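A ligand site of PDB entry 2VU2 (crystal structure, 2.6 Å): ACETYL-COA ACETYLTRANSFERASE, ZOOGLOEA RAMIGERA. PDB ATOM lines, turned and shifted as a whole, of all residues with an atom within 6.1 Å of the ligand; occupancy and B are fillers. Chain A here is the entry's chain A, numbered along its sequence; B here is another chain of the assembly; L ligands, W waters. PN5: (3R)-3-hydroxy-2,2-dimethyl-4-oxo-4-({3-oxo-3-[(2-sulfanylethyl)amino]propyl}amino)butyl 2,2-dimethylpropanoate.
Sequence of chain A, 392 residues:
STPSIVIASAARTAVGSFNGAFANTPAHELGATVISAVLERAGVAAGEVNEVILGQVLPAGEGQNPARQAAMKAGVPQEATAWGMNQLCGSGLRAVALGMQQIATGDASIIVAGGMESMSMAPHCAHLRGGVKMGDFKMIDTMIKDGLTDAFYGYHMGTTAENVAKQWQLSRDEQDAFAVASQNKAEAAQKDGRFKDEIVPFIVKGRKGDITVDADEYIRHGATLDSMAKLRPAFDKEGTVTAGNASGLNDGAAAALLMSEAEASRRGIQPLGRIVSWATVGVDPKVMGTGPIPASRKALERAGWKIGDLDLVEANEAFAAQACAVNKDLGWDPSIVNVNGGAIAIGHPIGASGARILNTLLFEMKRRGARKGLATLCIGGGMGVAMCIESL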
ATOM      1  N   PHE A  18      -4.752  -5.612   4.977  1.00  0.00           N
ATOM      2  CA  PHE A  18      -4.010  -5.474   6.191  1.00  0.00           C
ATOM      3  C   PHE A  18      -4.799  -6.211   7.244  1.00  0.00           C
ATOM      4  O   PHE A  18      -5.969  -5.936   7.448  1.00  0.00           O
ATOM      5  CB  PHE A  18      -3.817  -3.999   6.538  1.00  0.00           C
ATOM      6  CG  PHE A  18      -2.830  -3.765   7.628  1.00  0.00           C
ATOM      7  CD1 PHE A  18      -1.532  -4.279   7.533  1.00  0.00           C
ATOM      8  CD2 PHE A  18      -3.184  -3.047   8.765  1.00  0.00           C
ATOM      9  CE1 PHE A  18      -0.617  -4.095   8.553  1.00  0.00           C
ATOM     10  CE2 PHE A  18      -2.268  -2.849   9.783  1.00  0.00           C
ATOM     11  CZ  PHE A  18      -0.968  -3.372   9.668  1.00  0.00           C
ATOM     12  N   CYS A  89       9.940  -0.660  -2.400  1.00  0.00           N
ATOM     13  CA  CYS A  89       8.961  -0.996  -3.437  1.00  0.00           C
ATOM     14  C   CYS A  89       9.608  -1.667  -4.623  1.00  0.00           C
ATOM     15  O   CYS A  89       9.009  -2.545  -5.242  1.00  0.00           O
ATOM     16  CB  CYS A  89       8.231   0.261  -3.898  1.00  0.00           C
ATOM     17  SG  CYS A  89       7.731   1.317  -2.492  1.00  0.00           S
ATOM     18  N   GLY A 147       9.603   0.382   6.537  1.00  0.00           N
ATOM     19  CA  GLY A 147       8.985   0.254   5.211  1.00  0.00           C
ATOM     20  C   GLY A 147       8.420   1.546   4.655  1.00  0.00           C
ATOM     21  O   GLY A 147       8.625   1.850   3.488  1.00  0.00           O
ATOM     22  N   LEU A 148       7.747   2.334   5.499  1.00  0.00           N
ATOM     23  CA  LEU A 148       6.951   3.497   5.033  1.00  0.00           C
ATOM     24  C   LEU A 148       7.493   4.909   5.296  1.00  0.00           C
ATOM     25  O   LEU A 148       7.114   5.822   4.597  1.00  0.00           O
ATOM     26  CB  LEU A 148       5.556   3.451   5.685  1.00  0.00           C
ATOM     27  CG  LEU A 148       4.826   2.145   5.485  1.00  0.00           C
ATOM     28  CD1 LEU A 148       3.455   2.252   6.190  1.00  0.00           C
ATOM     29  CD2 LEU A 148       4.728   1.827   3.997  1.00  0.00           C
ATOM     30  N   HIS A 156       6.100  10.317   6.444  1.00  0.00           N
ATOM     31  CA  HIS A 156       5.528   9.163   5.748  1.00  0.00           C
ATOM     32  C   HIS A 156       5.714   9.362   4.243  1.00  0.00           C
ATOM     33  O   HIS A 156       5.852  10.499   3.771  1.00  0.00           O
ATOM     34  CB  HIS A 156       4.018   9.027   6.104  1.00  0.00           C
ATOM     35  CG  HIS A 156       3.433   7.665   5.869  1.00  0.00           C
ATOM     36  ND1 HIS A 156       2.983   6.868   6.911  1.00  0.00           N
ATOM     37  CD2 HIS A 156       3.171   6.980   4.730  1.00  0.00           C
ATOM     38  CE1 HIS A 156       2.490   5.740   6.415  1.00  0.00           C
ATOM     39  NE2 HIS A 156       2.593   5.782   5.097  1.00  0.00           N
ATOM     40  N   MET A 157       5.742   8.257   3.495  1.00  0.00           N
ATOM     41  CA  MET A 157       5.747   8.287   2.034  1.00  0.00           C
ATOM     42  C   MET A 157       4.646   9.215   1.453  1.00  0.00           C
ATOM     43  O   MET A 157       4.908   9.967   0.520  1.00  0.00           O
ATOM     44  CB  MET A 157       5.613   6.869   1.471  1.00  0.00           C
ATOM     45  CG  MET A 157       6.868   6.014   1.622  1.00  0.00           C
ATOM     46  SD  MET A 157       8.322   6.657   0.726  1.00  0.00           S
ATOM     47  CE  MET A 157       9.138   7.642   1.975  1.00  0.00           C
ATOM     48  N   GLY A 158       3.458   9.190   2.052  1.00  0.00           N
ATOM     49  CA  GLY A 158       2.339  10.060   1.650  1.00  0.00           C
ATOM     50  C   GLY A 158       2.650  11.548   1.504  1.00  0.00           C
ATOM     51  O   GLY A 158       2.052  12.225   0.639  1.00  0.00           O
ATOM     52  N   THR A 160       5.568  12.649   0.603  1.00  0.00           N
ATOM     53  CA  THR A 160       6.377  12.752  -0.608  1.00  0.00           C
ATOM     54  C   THR A 160       5.409  12.887  -1.770  1.00  0.00           C
ATOM     55  O   THR A 160       5.624  13.697  -2.679  1.00  0.00           O
ATOM     56  CB  THR A 160       7.374  11.550  -0.834  1.00  0.00           C
ATOM     57  OG1 THR A 160       6.675  10.364  -1.217  1.00  0.00           O
ATOM     58  CG2 THR A 160       8.230  11.269   0.399  1.00  0.00           C
ATOM     59  N   TYR A 218      -8.761  -6.867  -1.324  1.00  0.00           N
ATOM     60  CA  TYR A 218      -8.669  -5.442  -1.083  1.00  0.00           C
ATOM     61  C   TYR A 218      -9.441  -4.659  -2.145  1.00  0.00           C
ATOM     62  O   TYR A 218      -9.937  -3.560  -1.881  1.00  0.00           O
ATOM     63  CB  TYR A 218      -7.188  -5.053  -1.113  1.00  0.00           C
ATOM     64  CG  TYR A 218      -6.859  -3.629  -0.695  1.00  0.00           C
ATOM     65  CD1 TYR A 218      -7.184  -3.146   0.548  1.00  0.00           C
ATOM     66  CD2 TYR A 218      -6.154  -2.791  -1.559  1.00  0.00           C
ATOM     67  CE1 TYR A 218      -6.861  -1.855   0.928  1.00  0.00           C
ATOM     68  CE2 TYR A 218      -5.817  -1.510  -1.192  1.00  0.00           C
ATOM     69  CZ  TYR A 218      -6.168  -1.045   0.053  1.00  0.00           C
ATOM     70  OH  TYR A 218      -5.834   0.249   0.393  1.00  0.00           O
ATOM     71  N   ALA A 234      -5.069  12.138   4.562  1.00  0.00           N
ATOM     72  CA  ALA A 234      -4.465  11.189   5.494  1.00  0.00           C
ATOM     73  C   ALA A 234      -3.183  11.719   6.117  1.00  0.00           C
ATOM     74  O   ALA A 234      -2.868  11.404   7.261  1.00  0.00           O
ATOM     75  CB  ALA A 234      -4.201   9.840   4.794  1.00  0.00           C
ATOM     76  N   PHE A 235      -2.439  12.536   5.365  1.00  0.00           N
ATOM     77  CA  PHE A 235      -1.131  13.008   5.810  1.00  0.00           C
ATOM     78  C   PHE A 235      -1.144  14.515   6.100  1.00  0.00           C
ATOM     79  O   PHE A 235      -1.197  14.909   7.272  1.00  0.00           O
ATOM     80  CB  PHE A 235      -0.079  12.622   4.766  1.00  0.00           C
ATOM     81  CG  PHE A 235      -0.226  11.215   4.297  1.00  0.00           C
ATOM     82  CD1 PHE A 235       0.216  10.155   5.093  1.00  0.00           C
ATOM     83  CD2 PHE A 235      -0.841  10.936   3.097  1.00  0.00           C
ATOM     84  CE1 PHE A 235       0.080   8.839   4.681  1.00  0.00           C
ATOM     85  CE2 PHE A 235      -0.988   9.605   2.671  1.00  0.00           C
ATOM     86  CZ  PHE A 235      -0.528   8.557   3.463  1.00  0.00           C
ATOM     87  N   THR A 242      -5.162  11.065   0.209  1.00  0.00           N
ATOM     88  CA  THR A 242      -6.059  10.411   1.188  1.00  0.00           C
ATOM     89  C   THR A 242      -5.800   8.898   1.236  1.00  0.00           C
ATOM     90  O   THR A 242      -5.019   8.402   0.485  1.00  0.00           O
ATOM     91  CB  THR A 242      -7.561  10.649   0.831  1.00  0.00           C
ATOM     92  OG1 THR A 242      -7.903   9.877  -0.332  1.00  0.00           O
ATOM     93  CG2 THR A 242      -7.846  12.113   0.567  1.00  0.00           C
ATOM     94  N   ALA A 243      -6.497   8.183   2.117  1.00  0.00           N
ATOM     95  CA  ALA A 243      -6.448   6.727   2.136  1.00  0.00           C
ATOM     96  C   ALA A 243      -7.115   6.175   0.877  1.00  0.00           C
ATOM     97  O   ALA A 243      -6.777   5.089   0.370  1.00  0.00           O
ATOM     98  CB  ALA A 243      -7.125   6.187   3.410  1.00  0.00           C
ATOM     99  N   ALA A 246      -4.443   6.719  -2.022  1.00  0.00           N
ATOM    100  CA  ALA A 246      -3.189   6.086  -1.673  1.00  0.00           C
ATOM    101  C   ALA A 246      -3.369   4.595  -1.755  1.00  0.00           C
ATOM    102  O   ALA A 246      -4.495   4.097  -1.643  1.00  0.00           O
ATOM    103  CB  ALA A 246      -2.758   6.471  -0.286  1.00  0.00           C
ATOM    104  N   SER A 247      -2.275   3.868  -1.989  1.00  0.00           N
ATOM    105  CA  SER A 247      -2.320   2.415  -1.903  1.00  0.00           C
ATOM    106  C   SER A 247      -2.483   2.038  -0.437  1.00  0.00           C
ATOM    107  O   SER A 247      -2.572   2.910   0.475  1.00  0.00           O
ATOM    108  CB  SER A 247      -1.062   1.766  -2.441  1.00  0.00           C
ATOM    109  OG  SER A 247      -1.357   0.418  -2.788  1.00  0.00           O
ATOM    110  N   GLY A 248      -2.538   0.730  -0.211  1.00  0.00           N
ATOM    111  CA  GLY A 248      -2.760   0.223   1.114  1.00  0.00           C
ATOM    112  C   GLY A 248      -1.563  -0.502   1.685  1.00  0.00           C
ATOM    113  O   GLY A 248      -0.475  -0.546   1.073  1.00  0.00           O
ATOM    114  N   LEU A 249      -1.836  -1.093   2.844  1.00  0.00           N
ATOM    115  CA  LEU A 249      -0.953  -2.014   3.522  1.00  0.00           C
ATOM    116  C   LEU A 249      -1.428  -3.442   3.182  1.00  0.00           C
ATOM    117  O   LEU A 249      -2.574  -3.777   3.404  1.00  0.00           O
ATOM    118  CB  LEU A 249      -1.001  -1.713   5.034  1.00  0.00           C
ATOM    119  CG  LEU A 249      -0.868  -0.203   5.381  1.00  0.00           C
ATOM    120  CD1 LEU A 249      -1.466   0.126   6.700  1.00  0.00           C
ATOM    121  CD2 LEU A 249       0.611   0.344   5.292  1.00  0.00           C
ATOM    122  N   MET A 288      10.018  11.106  -4.381  1.00  0.00           N
ATOM    123  CA  MET A 288      10.392   9.715  -4.689  1.00  0.00           C
ATOM    124  C   MET A 288       9.434   9.026  -5.650  1.00  0.00           C
ATOM    125  O   MET A 288       9.826   8.091  -6.367  1.00  0.00           O
ATOM    126  CB  MET A 288      10.489   8.889  -3.399  1.00  0.00           C
ATOM    127  CG  MET A 288       9.159   8.477  -2.816  1.00  0.00           C
ATOM    128  SD  MET A 288       8.423   7.003  -3.604  1.00  0.00           S
ATOM    129  CE  MET A 288       6.787   7.114  -2.868  1.00  0.00           C
ATOM    130  N   ASN A 316       3.226   1.025 -11.370  1.00  0.00           N
ATOM    131  CA  ASN A 316       2.682   0.878 -10.029  1.00  0.00           C
ATOM    132  C   ASN A 316       2.014   2.145  -9.448  1.00  0.00           C
ATOM    133  O   ASN A 316       2.526   3.261  -9.587  1.00  0.00           O
ATOM    134  CB  ASN A 316       3.750   0.396  -9.055  1.00  0.00           C
ATOM    135  CG  ASN A 316       3.171  -0.066  -7.748  1.00  0.00           C
ATOM    136  OD1 ASN A 316       2.340  -0.992  -7.720  1.00  0.00           O
ATOM    137  ND2 ASN A 316       3.613   0.559  -6.649  1.00  0.00           N
ATOM    138  N   ALA A 318       1.536   3.738  -6.335  1.00  0.00           N
ATOM    139  CA  ALA A 318       1.843   4.009  -4.932  1.00  0.00           C
ATOM    140  C   ALA A 318       0.903   5.095  -4.460  1.00  0.00           C
ATOM    141  O   ALA A 318       0.231   4.938  -3.478  1.00  0.00           O
ATOM    142  CB  ALA A 318       3.295   4.451  -4.761  1.00  0.00           C
ATOM    143  N   PHE A 319       0.882   6.202  -5.180  1.00  0.00           N
ATOM    144  CA  PHE A 319      -0.120   7.269  -4.945  1.00  0.00           C
ATOM    145  C   PHE A 319      -0.696   7.780  -6.274  1.00  0.00           C
ATOM    146  O   PHE A 319       0.005   7.824  -7.281  1.00  0.00           O
ATOM    147  CB  PHE A 319       0.498   8.435  -4.163  1.00  0.00           C
ATOM    148  CG  PHE A 319       1.067   8.030  -2.854  1.00  0.00           C
ATOM    149  CD1 PHE A 319       0.292   8.095  -1.709  1.00  0.00           C
ATOM    150  CD2 PHE A 319       2.351   7.530  -2.768  1.00  0.00           C
ATOM    151  CE1 PHE A 319       0.809   7.687  -0.490  1.00  0.00           C
ATOM    152  CE2 PHE A 319       2.860   7.121  -1.564  1.00  0.00           C
ATOM    153  CZ  PHE A 319       2.092   7.193  -0.417  1.00  0.00           C
ATOM    154  N   HIS A 348      -0.530  -3.201  -2.031  1.00  0.00           N
ATOM    155  CA  HIS A 348       0.885  -2.946  -2.171  1.00  0.00           C
ATOM    156  C   HIS A 348       1.670  -3.733  -1.136  1.00  0.00           C
ATOM    157  O   HIS A 348       2.009  -3.208  -0.081  1.00  0.00           O
ATOM    158  CB  HIS A 348       1.144  -1.451  -2.042  1.00  0.00           C
ATOM    159  CG  HIS A 348       2.531  -1.053  -2.418  1.00  0.00           C
ATOM    160  ND1 HIS A 348       3.132  -1.486  -3.575  1.00  0.00           N
ATOM    161  CD2 HIS A 348       3.456  -0.315  -1.760  1.00  0.00           C
ATOM    162  CE1 HIS A 348       4.359  -1.008  -3.637  1.00  0.00           C
ATOM    163  NE2 HIS A 348       4.587  -0.302  -2.539  1.00  0.00           N
ATOM    164  N   ILE A 350       4.779  -4.471  -0.086  1.00  0.00           N
ATOM    165  CA  ILE A 350       6.008  -3.705  -0.460  1.00  0.00           C
ATOM    166  C   ILE A 350       7.033  -4.543  -1.210  1.00  0.00           C
ATOM    167  O   ILE A 350       7.360  -4.220  -2.335  1.00  0.00           O
ATOM    168  CB  ILE A 350       6.677  -3.006   0.765  1.00  0.00           C
ATOM    169  CG1 ILE A 350       5.775  -1.932   1.368  1.00  0.00           C
ATOM    170  CG2 ILE A 350       7.939  -2.287   0.380  1.00  0.00           C
ATOM    171  CD1 ILE A 350       6.347  -1.311   2.639  1.00  0.00           C
ATOM    172  N   CYS A 378       7.925   3.115  -8.413  1.00  0.00           N
ATOM    173  CA  CYS A 378       8.622   4.121  -7.635  1.00  0.00           C
ATOM    174  C   CYS A 378       9.133   3.487  -6.317  1.00  0.00           C
ATOM    175  O   CYS A 378       8.571   2.515  -5.823  1.00  0.00           O
ATOM    176  CB  CYS A 378       7.713   5.327  -7.346  1.00  0.00           C
ATOM    177  SG  CYS A 378       6.445   5.034  -6.118  1.00  0.00           S
ATOM    178  N   GLY A 380      10.843   4.155  -2.319  1.00  0.00           N
ATOM    179  CA  GLY A 380      11.117   5.005  -1.167  1.00  0.00           C
ATOM    180  C   GLY A 380      12.584   5.278  -1.085  1.00  0.00           C
ATOM    181  O   GLY A 380      13.383   4.548  -1.656  1.00  0.00           O
ATOM    182  N   MET B 134      -1.882  -0.647  14.294  1.00  0.00           N
ATOM    183  CA  MET B 134      -0.879   0.122  13.569  1.00  0.00           C
ATOM    184  C   MET B 134      -0.378   1.281  14.432  1.00  0.00           C
ATOM    185  O   MET B 134      -1.160   1.915  15.138  1.00  0.00           O
ATOM    186  CB  MET B 134      -1.511   0.650  12.278  1.00  0.00           C
ATOM    187  CG  MET B 134      -0.566   1.293  11.312  1.00  0.00           C
ATOM    188  SD  MET B 134      -1.417   2.358  10.124  1.00  0.00           S
ATOM    189  CE  MET B 134      -2.994   1.564   9.873  1.00  0.00           C
HETATM  190  CP2 PN5 L   1       4.654   2.780  -1.269  1.00  0.00           C
HETATM  191  CP3 PN5 L   1       4.296   2.466   0.185  1.00  0.00           C
HETATM  192  NP4 PN5 L   1       2.851   2.647   0.298  1.00  0.00           N
HETATM  193  CP5 PN5 L   1       2.222   3.598   0.969  1.00  0.00           C
HETATM  194  OP5 PN5 L   1       2.809   4.477   1.582  1.00  0.00           O
HETATM  195  CP6 PN5 L   1       0.705   3.554   0.906  1.00  0.00           C
HETATM  196  CP7 PN5 L   1       0.131   2.898   2.146  1.00  0.00           C
HETATM  197  NP8 PN5 L   1      -0.438   3.953   2.985  1.00  0.00           N
HETATM  198  CP9 PN5 L   1      -1.565   3.932   3.690  1.00  0.00           C
HETATM  199  OP9 PN5 L   1      -2.327   2.967   3.700  1.00  0.00           O
HETATM  200  CPA PN5 L   1      -1.858   5.198   4.456  1.00  0.00           C
HETATM  201  OPA PN5 L   1      -0.618   5.686   4.978  1.00  0.00           O
HETATM  202  CPB PN5 L   1      -2.823   5.008   5.620  1.00  0.00           C
HETATM  203  CPE PN5 L   1      -2.896   6.305   6.439  1.00  0.00           C
HETATM  204  CPD PN5 L   1      -2.337   3.882   6.514  1.00  0.00           C
HETATM  205  CPC PN5 L   1      -4.238   4.725   5.096  1.00  0.00           C
HETATM  206  OA6 PN5 L   1      -4.653   3.405   5.435  1.00  0.00           O
HETATM  207  CT1 PN5 L   1      -5.319   3.142   6.704  1.00  0.00           C
HETATM  208  OT1 PN5 L   1      -5.305   3.991   7.579  1.00  0.00           O
HETATM  209  CT2 PN5 L   1      -5.992   1.810   6.925  1.00  0.00           C
HETATM  210  CT5 PN5 L   1      -5.768   1.381   8.378  1.00  0.00           C
HETATM  211  CT3 PN5 L   1      -5.368   0.795   5.972  1.00  0.00           C
HETATM  212  CT4 PN5 L   1      -7.488   1.984   6.647  1.00  0.00           C
HETATM  213  SP1 PN5 L   1       5.303   4.459  -1.411  1.00  0.00           S
HETATM  214  O   HOH W   1      -0.305   5.906   7.518  1.00  0.00           O
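N of Met 157 lies close to O of Leu 148 (3.0 Å).
The side-chain sulfur (SD) of Met 288 sits at hydrogen-bond distance from the side-chain sulfur (SG) of Cys 378.
N of Ser 247 is in hydrogen-bond range of O of Ala 318 (3.1 Å).
The backbone carbonyl oxygen of Met 157 sits at hydrogen-bond distance from the side-chain hydroxyl of Thr 160 (2.5 Å).
The backbone NH of Gly 248 lies close to the side-chain hydroxyl of Tyr 218 (3.4 Å).
O of Leu 249 sits at hydrogen-bond distance from N of Phe 18.
The backbone carbonyl oxygen (O) of Cys 378 lies close to the side-chain sulfur (SG) of Cys 89.
A ring nitrogen (NE2) of His 348 is in hydrogen-bond range of the side-chain sulfur (SG) of Cys 89.
Merely in contact with the ligand: Cys 89, Leu 148, Met 157, Phe 235, Ala 243, Gly 248, Leu 249, Met 288, Ala 318, Phe 319, His 348 and Met 134 of chain B.
Of the 26 residues printed, 14 come within 4 Å of the ligand.
Water W1 lies within hydrogen-bond range of an oxygen (OPA) of the ligand (2.6 Å) and a ring nitrogen (ND1) of His 156 (3.5 Å).
A ring nitrogen (NE2) of His 156 is in hydrogen-bond range of an oxygen (OPA) of the ligand (3.2 Å).
A nitrogen (NP8) of the ligand lies close to the backbone carbonyl oxygen (O) of Ser 247, 3.5 Å away.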
